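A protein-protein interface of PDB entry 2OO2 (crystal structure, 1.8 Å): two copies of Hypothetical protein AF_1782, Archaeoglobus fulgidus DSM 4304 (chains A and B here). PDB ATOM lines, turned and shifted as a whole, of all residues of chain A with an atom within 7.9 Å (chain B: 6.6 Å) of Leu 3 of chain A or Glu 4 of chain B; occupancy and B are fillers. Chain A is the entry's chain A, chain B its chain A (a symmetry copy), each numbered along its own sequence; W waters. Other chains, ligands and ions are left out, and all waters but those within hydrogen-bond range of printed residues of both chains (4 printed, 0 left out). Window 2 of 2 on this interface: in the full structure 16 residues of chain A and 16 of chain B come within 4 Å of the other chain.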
ATOM      1  N   SER A   2      21.938   4.687 -20.592  1.00  0.00           N
ATOM      2  CA  SER A   2      21.021   3.830 -19.784  1.00  0.00           C
ATOM      3  C   SER A   2      19.874   3.205 -20.578  1.00  0.00           C
ATOM      4  O   SER A   2      19.632   2.006 -20.454  1.00  0.00           O
ATOM      5  CB  SER A   2      20.410   4.554 -18.621  1.00  0.00           C
ATOM      6  OG  SER A   2      19.698   3.562 -17.869  1.00  0.00           O
ATOM      7  N   LEU A   3      19.144   4.010 -21.347  1.00  0.00           N
ATOM      8  CA  LEU A   3      18.337   3.445 -22.419  1.00  0.00           C
ATOM      9  C   LEU A   3      19.256   2.829 -23.490  1.00  0.00           C
ATOM     10  O   LEU A   3      18.939   1.780 -24.077  1.00  0.00           O
ATOM     11  CB  LEU A   3      17.403   4.503 -23.003  1.00  0.00           C
ATOM     12  CG  LEU A   3      16.099   4.042 -23.654  1.00  0.00           C
ATOM     13  CD1 LEU A   3      15.373   3.081 -22.758  1.00  0.00           C
ATOM     14  CD2 LEU A   3      15.192   5.225 -23.983  1.00  0.00           C
ATOM     15  N   GLU A   4      20.412   3.443 -23.732  1.00  0.00           N
ATOM     16  CA  GLU A   4      21.403   2.901 -24.679  1.00  0.00           C
ATOM     17  C   GLU A   4      21.957   1.606 -24.148  1.00  0.00           C
ATOM     18  O   GLU A   4      22.113   0.646 -24.890  1.00  0.00           O
ATOM     19  CB  GLU A   4      22.591   3.838 -24.887  1.00  0.00           C
ATOM     20  CG  GLU A   4      22.236   5.292 -24.837  1.00  0.00           C
ATOM     21  CD  GLU A   4      23.128   6.126 -25.765  1.00  0.00           C
ATOM     22  OE1 GLU A   4      24.372   5.870 -25.782  1.00  0.00           O
ATOM     23  OE2 GLU A   4      22.563   7.021 -26.468  1.00  0.00           O
ATOM     24  N   GLU A   5      22.314   1.632 -22.864  1.00  0.00           N
ATOM     25  CA  GLU A   5      22.706   0.442 -22.086  1.00  0.00           C
ATOM     26  C   GLU A   5      21.665  -0.693 -22.117  1.00  0.00           C
ATOM     27  O   GLU A   5      22.018  -1.821 -22.365  1.00  0.00           O
ATOM     28  CB  GLU A   5      22.990   0.856 -20.642  1.00  0.00           C
ATOM     29  CG  GLU A   5      23.374  -0.257 -19.690  1.00  0.00           C
ATOM     30  CD  GLU A   5      23.880   0.296 -18.334  1.00  0.00           C
ATOM     31  OE1 GLU A   5      23.357  -0.135 -17.270  1.00  0.00           O
ATOM     32  OE2 GLU A   5      24.778   1.188 -18.351  1.00  0.00           O
ATOM     33  N   GLU A   6      20.399  -0.373 -21.877  1.00  0.00           N
ATOM     34  CA  GLU A   6      19.356  -1.366 -21.844  1.00  0.00           C
ATOM     35  C   GLU A   6      19.210  -2.005 -23.247  1.00  0.00           C
ATOM     36  O   GLU A   6      19.207  -3.226 -23.343  1.00  0.00           O
ATOM     37  CB  GLU A   6      18.026  -0.808 -21.305  1.00  0.00           C
ATOM     38  CG  GLU A   6      17.013  -1.947 -21.064  1.00  0.00           C
ATOM     39  CD  GLU A   6      15.570  -1.527 -20.686  1.00  0.00           C
ATOM     40  OE1 GLU A   6      15.262  -0.311 -20.544  1.00  0.00           O
ATOM     41  OE2 GLU A   6      14.726  -2.467 -20.539  1.00  0.00           O
ATOM     42  N   LEU A   7      19.149  -1.200 -24.314  1.00  0.00           N
ATOM     43  CA  LEU A   7      19.058  -1.759 -25.706  1.00  0.00           C
ATOM     44  C   LEU A   7      20.261  -2.587 -26.162  1.00  0.00           C
ATOM     45  O   LEU A   7      20.115  -3.576 -26.846  1.00  0.00           O
ATOM     46  CB  LEU A   7      18.803  -0.671 -26.770  1.00  0.00           C
ATOM     47  CG  LEU A   7      17.447  -0.067 -27.037  1.00  0.00           C
ATOM     48  CD1 LEU A   7      17.617   1.050 -28.004  1.00  0.00           C
ATOM     49  CD2 LEU A   7      16.501  -1.129 -27.625  1.00  0.00           C
ATOM     50  N   ARG A   8      21.468  -2.133 -25.863  1.00  0.00           N
ATOM     51  CA  ARG A   8      22.674  -2.892 -26.117  1.00  0.00           C
ATOM     52  C   ARG A   8      22.681  -4.209 -25.396  1.00  0.00           C
ATOM     53  O   ARG A   8      22.971  -5.228 -26.043  1.00  0.00           O
ATOM     54  CB  ARG A   8      23.928  -2.133 -25.641  1.00  0.00           C
ATOM     55  CG  ARG A   8      24.475  -1.220 -26.640  1.00  0.00           C
ATOM     56  CD  ARG A   8      25.910  -0.853 -26.264  1.00  0.00           C
ATOM     57  NE  ARG A   8      26.108   0.568 -26.553  1.00  0.00           N
ATOM     58  CZ  ARG A   8      26.179   1.523 -25.619  1.00  0.00           C
ATOM     59  NH1 ARG A   8      26.084   1.217 -24.315  1.00  0.00           N
ATOM     60  NH2 ARG A   8      26.353   2.799 -25.988  1.00  0.00           N
ATOM     61  N   ARG A   9      22.364  -4.224 -24.093  1.00  0.00           N
ATOM     62  CA  ARG A   9      22.422  -5.460 -23.304  1.00  0.00           C
ATOM     63  C   ARG A   9      21.416  -6.486 -23.899  1.00  0.00           C
ATOM     64  O   ARG A   9      21.764  -7.636 -24.024  1.00  0.00           O
ATOM     65  CB  ARG A   9      22.068  -5.290 -21.830  1.00  0.00           C
ATOM     66  CG  ARG A   9      23.113  -4.454 -21.083  1.00  0.00           C
ATOM     67  CD  ARG A   9      23.386  -4.927 -19.653  1.00  0.00           C
ATOM     68  NE  ARG A   9      24.287  -3.953 -19.032  1.00  0.00           N
ATOM     69  CZ  ARG A   9      23.925  -3.091 -18.082  1.00  0.00           C
ATOM     70  NH1 ARG A   9      22.675  -3.097 -17.601  1.00  0.00           N
ATOM     71  NH2 ARG A   9      24.823  -2.229 -17.599  1.00  0.00           N
ATOM     72  N   LEU A  51      20.989   1.198 -32.652  1.00  0.00           N
ATOM     73  CA  LEU A  51      20.412   0.281 -31.618  1.00  0.00           C
ATOM     74  C   LEU A  51      18.954  -0.088 -31.821  1.00  0.00           C
ATOM     75  O   LEU A  51      18.596  -1.328 -31.692  1.00  0.00           O
ATOM     76  CB  LEU A  51      20.644   0.825 -30.200  1.00  0.00           C
ATOM     77  CG  LEU A  51      22.119   0.916 -29.860  1.00  0.00           C
ATOM     78  CD1 LEU A  51      22.221   1.541 -28.445  1.00  0.00           C
ATOM     79  CD2 LEU A  51      22.820  -0.406 -29.877  1.00  0.00           C
ATOM     80  N   VAL A  52      18.138   0.888 -32.227  1.00  0.00           N
ATOM     81  CA  VAL A  52      16.698   0.606 -32.406  1.00  0.00           C
ATOM     82  C   VAL A  52      16.572  -0.417 -33.553  1.00  0.00           C
ATOM     83  O   VAL A  52      15.820  -1.447 -33.420  1.00  0.00           O
ATOM     84  CB  VAL A  52      15.898   1.833 -32.814  1.00  0.00           C
ATOM     85  CG1 VAL A  52      14.469   1.542 -32.880  1.00  0.00           C
ATOM     86  CG2 VAL A  52      16.030   2.940 -31.714  1.00  0.00           C
ATOM     87  N   SER B   2      16.598  11.492 -27.109  1.00  0.00           N
ATOM     88  CA  SER B   2      16.875  11.236 -28.554  1.00  0.00           C
ATOM     89  C   SER B   2      16.813   9.764 -28.960  1.00  0.00           C
ATOM     90  O   SER B   2      16.175   9.435 -29.958  1.00  0.00           O
ATOM     91  CB  SER B   2      18.205  11.762 -29.002  1.00  0.00           C
ATOM     92  OG  SER B   2      18.242  11.582 -30.424  1.00  0.00           O
ATOM     93  N   LEU B   3      17.504   8.893 -28.229  1.00  0.00           N
ATOM     94  CA  LEU B   3      17.169   7.476 -28.290  1.00  0.00           C
ATOM     95  C   LEU B   3      15.764   7.250 -27.701  1.00  0.00           C
ATOM     96  O   LEU B   3      14.992   6.409 -28.195  1.00  0.00           O
ATOM     97  CB  LEU B   3      18.232   6.642 -27.578  1.00  0.00           C
ATOM     98  CG  LEU B   3      18.436   5.193 -28.019  1.00  0.00           C
ATOM     99  CD1 LEU B   3      18.559   5.109 -29.513  1.00  0.00           C
ATOM    100  CD2 LEU B   3      19.670   4.579 -27.365  1.00  0.00           C
ATOM    101  N   GLU B   4      15.402   8.012 -26.671  1.00  0.00           N
ATOM    102  CA  GLU B   4      14.055   7.935 -26.078  1.00  0.00           C
ATOM    103  C   GLU B   4      13.034   8.421 -27.072  1.00  0.00           C
ATOM    104  O   GLU B   4      11.979   7.820 -27.223  1.00  0.00           O
ATOM    105  CB  GLU B   4      13.910   8.810 -24.834  1.00  0.00           C
ATOM    106  CG  GLU B   4      15.153   8.897 -24.003  1.00  0.00           C
ATOM    107  CD  GLU B   4      14.829   9.048 -22.512  1.00  0.00           C
ATOM    108  OE1 GLU B   4      13.898   9.848 -22.183  1.00  0.00           O
ATOM    109  OE2 GLU B   4      15.511   8.354 -21.693  1.00  0.00           O
ATOM    110  N   GLU B   5      13.348   9.559 -27.690  1.00  0.00           N
ATOM    111  CA  GLU B   5      12.596  10.124 -28.826  1.00  0.00           C
ATOM    112  C   GLU B   5      12.419   9.146 -30.003  1.00  0.00           C
ATOM    113  O   GLU B   5      11.325   8.990 -30.491  1.00  0.00           O
ATOM    114  CB  GLU B   5      13.287  11.402 -29.302  1.00  0.00           C
ATOM    115  CG  GLU B   5      12.662  12.097 -30.493  1.00  0.00           C
ATOM    116  CD  GLU B   5      13.281  13.497 -30.733  1.00  0.00           C
ATOM    117  OE1 GLU B   5      13.718  13.779 -31.882  1.00  0.00           O
ATOM    118  OE2 GLU B   5      13.355  14.292 -29.750  1.00  0.00           O
ATOM    119  N   GLU B   6      13.496   8.498 -30.432  1.00  0.00           N
ATOM    120  CA  GLU B   6      13.444   7.593 -31.550  1.00  0.00           C
ATOM    121  C   GLU B   6      12.531   6.393 -31.199  1.00  0.00           C
ATOM    122  O   GLU B   6      11.646   6.074 -31.984  1.00  0.00           O
ATOM    123  CB  GLU B   6      14.844   7.156 -32.020  1.00  0.00           C
ATOM    124  CG  GLU B   6      14.756   6.384 -33.354  1.00  0.00           C
ATOM    125  CD  GLU B   6      16.064   5.728 -33.867  1.00  0.00           C
ATOM    126  OE1 GLU B   6      17.149   5.862 -33.236  1.00  0.00           O
ATOM    127  OE2 GLU B   6      15.975   5.051 -34.939  1.00  0.00           O
ATOM    128  N   LEU B   7      12.703   5.781 -30.022  1.00  0.00           N
ATOM    129  CA  LEU B   7      11.816   4.643 -29.601  1.00  0.00           C
ATOM    130  C   LEU B   7      10.338   4.994 -29.417  1.00  0.00           C
ATOM    131  O   LEU B   7       9.467   4.218 -29.743  1.00  0.00           O
ATOM    132  CB  LEU B   7      12.302   3.956 -28.308  1.00  0.00           C
ATOM    133  CG  LEU B   7      13.429   2.953 -28.268  1.00  0.00           C
ATOM    134  CD1 LEU B   7      13.718   2.633 -26.845  1.00  0.00           C
ATOM    135  CD2 LEU B   7      13.024   1.673 -29.020  1.00  0.00           C
ATOM    136  N   ARG B   8      10.049   6.131 -28.806  1.00  0.00           N
ATOM    137  CA  ARG B   8       8.697   6.638 -28.696  1.00  0.00           C
ATOM    138  C   ARG B   8       8.065   6.869 -30.038  1.00  0.00           C
ATOM    139  O   ARG B   8       6.926   6.416 -30.233  1.00  0.00           O
ATOM    140  CB  ARG B   8       8.662   7.993 -27.963  1.00  0.00           C
ATOM    141  CG  ARG B   8       8.571   7.872 -26.511  1.00  0.00           C
ATOM    142  CD  ARG B   8       8.115   9.203 -25.916  1.00  0.00           C
ATOM    143  NE  ARG B   8       8.868   9.434 -24.681  1.00  0.00           N
ATOM    144  CZ  ARG B   8       9.860  10.322 -24.561  1.00  0.00           C
ATOM    145  NH1 ARG B   8      10.222  11.093 -25.600  1.00  0.00           N
ATOM    146  NH2 ARG B   8      10.496  10.451 -23.388  1.00  0.00           N
ATOM    147  N   ARG B   9       8.763   7.545 -30.963  1.00  0.00           N
ATOM    148  CA  ARG B   9       8.182   7.876 -32.270  1.00  0.00           C
ATOM    149  C   ARG B   9       7.837   6.556 -33.017  1.00  0.00           C
ATOM    150  O   ARG B   9       6.779   6.475 -33.596  1.00  0.00           O
ATOM    151  CB  ARG B   9       9.098   8.680 -33.187  1.00  0.00           C
ATOM    152  CG  ARG B   9       9.349  10.094 -32.647  1.00  0.00           C
ATOM    153  CD  ARG B   9       9.425  11.172 -33.730  1.00  0.00           C
ATOM    154  NE  ARG B   9       9.808  12.426 -33.078  1.00  0.00           N
ATOM    155  CZ  ARG B   9      11.001  13.006 -33.202  1.00  0.00           C
ATOM    156  NH1 ARG B   9      11.938  12.469 -33.994  1.00  0.00           N
ATOM    157  NH2 ARG B   9      11.253  14.140 -32.544  1.00  0.00           N
ATOM    158  N   GLY B  49       6.054   4.142 -19.678  1.00  0.00           N
ATOM    159  CA  GLY B  49       7.438   4.503 -20.050  1.00  0.00           C
ATOM    160  C   GLY B  49       8.425   3.357 -20.110  1.00  0.00           C
ATOM    161  O   GLY B  49       9.614   3.564 -20.016  1.00  0.00           O
ATOM    162  N   LEU B  51       9.952   1.802 -22.588  1.00  0.00           N
ATOM    163  CA  LEU B  51      10.072   1.926 -24.076  1.00  0.00           C
ATOM    164  C   LEU B  51      10.609   0.697 -24.786  1.00  0.00           C
ATOM    165  O   LEU B  51      10.014   0.282 -25.862  1.00  0.00           O
ATOM    166  CB  LEU B  51      10.874   3.177 -24.467  1.00  0.00           C
ATOM    167  CG  LEU B  51      10.188   4.455 -24.024  1.00  0.00           C
ATOM    168  CD1 LEU B  51      11.123   5.628 -24.410  1.00  0.00           C
ATOM    169  CD2 LEU B  51       8.842   4.658 -24.647  1.00  0.00           C
ATOM    170  N   VAL B  52      11.615   0.051 -24.192  1.00  0.00           N
ATOM    171  CA  VAL B  52      12.212  -1.130 -24.850  1.00  0.00           C
ATOM    172  C   VAL B  52      11.121  -2.219 -24.910  1.00  0.00           C
ATOM    173  O   VAL B  52      10.910  -2.861 -26.000  1.00  0.00           O
ATOM    174  CB  VAL B  52      13.381  -1.716 -24.075  1.00  0.00           C
ATOM    175  CG1 VAL B  52      14.010  -2.814 -24.803  1.00  0.00           C
ATOM    176  CG2 VAL B  52      14.508  -0.639 -23.925  1.00  0.00           C
HETATM  177  O   HOH W   1      12.719   0.873 -21.463  1.00  0.00           O
HETATM  178  O   HOH W   2      20.207   8.818 -26.636  1.00  0.00           O
HETATM  179  O   HOH W   3      18.104   6.971 -21.289  1.00  0.00           O
HETATM  180  O   HOH W   4      19.131   3.705 -32.875  1.00  0.00           O
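OE1 of Glu 4 of chain A lies within salt-bridge range of NH2 of Arg 8 of chain A (3.7 Å). The guanidinium group of Arg 8 of chain B lies within salt-bridge range of the side-chain carboxylate of Glu 4 of chain B (3.7 Å).
Among the printed residues, merely in contact across the chains: Leu 3 of chain A with Glu 4 of chain B (3.6 Å), Leu 3 of chain A with Val 52 of chain B (3.99 Å), Glu 4 of chain A with Leu 3 of chain B (3.6 Å), Glu 6 of chain A with Val 52 of chain B (3.5 Å), Val 52 of chain A with Leu 3 of chain B (3.99 Å) and Val 52 of chain A with Glu 6 of chain B (3.5 Å).
Of the printed residues of chain B, Leu 3 of chain A touches Glu 4 (3.6 Å) and Val 52 (3.99 Å). Of the printed residues of chain B, Glu 6 of chain A touches Val 52. Leu 7 of chain A touches none of the printed residues of chain B. Of the printed residues of chain B, Val 52 of chain A touches Leu 3 and Glu 6. Of the printed residues of chain A, Leu 3 of chain B touches Glu 4 (3.6 Å) and Val 52 (3.99 Å). Glu 4 of chain B touches just one residue of chain A: Leu 3. Of the printed residues of chain A, Glu 6 of chain B touches Val 52 (3.5 Å). Gly 49 of chain B touches none of the printed residues of chain A. Of the printed residues of chain A, Val 52 of chain B touches Leu 3 (3.99 Å) and Glu 6 (3.5 Å). The nearest printed residue of chain B that does not touch Leu 3 of chain A is Leu 51 of chain B (4.1 Å). The nearest printed residue of chain A that does not touch Val 52 of chain B is Leu 7 of chain A (4.1 Å).
Printed residues of chain B that touch a printed residue of chain A: Leu 3, Glu 4, Glu 6 and Val 52. Hydrophobic or aromatic side chains of chain B within 4 Å of the printed part of chain A: Leu 3 and Val 52. Of the 10 printed residues of chain A, 4 touch a printed residue of chain B. Hydrophobic or aromatic side chains of chain A that line the printed part of chain B: Leu 3 and Val 52. Among the printed residues, 6 pairs touch across the chains. Among the printed residues, no Asp or Glu carboxylate lies within 4 Å of a Lys or Arg side-chain nitrogen of the other chain.
Leu 3 of chain A touches Glu 4 of chain B, and with the chains exchanged Glu 4 of chain A touches Leu 3 of chain B. Leu 3 of chain A touches Val 52 of chain B, and with the chains exchanged Val 52 of chain A touches Leu 3 of chain B. Glu 6 of chain A touches Val 52 of chain B, and with the chains exchanged Val 52 of chain A touches Glu 6 of chain B.
Water W1 lies within hydrogen-bond range of OE1 of Glu 6 of chain A (3.0 Å), N of Val 52 of chain B (3.1 Å) and N of Leu 51 of chain B (3.1 Å). Water W4 lies within hydrogen-bond range of OE1 of Glu 6 of chain B, N of Val 52 of chain A and N of Leu 51 of chain A. Water W3 bridges OE2 of Glu 4 of chain B (3.0 Å) and N of Leu 3 of chain A (3.1 Å). Water W2 lies within hydrogen-bond range of the side-chain carboxylate (OE2) of Glu 4 of chain A (3.0 Å) and the backbone NH (N) of Leu 3 of chain B (3.1 Å).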
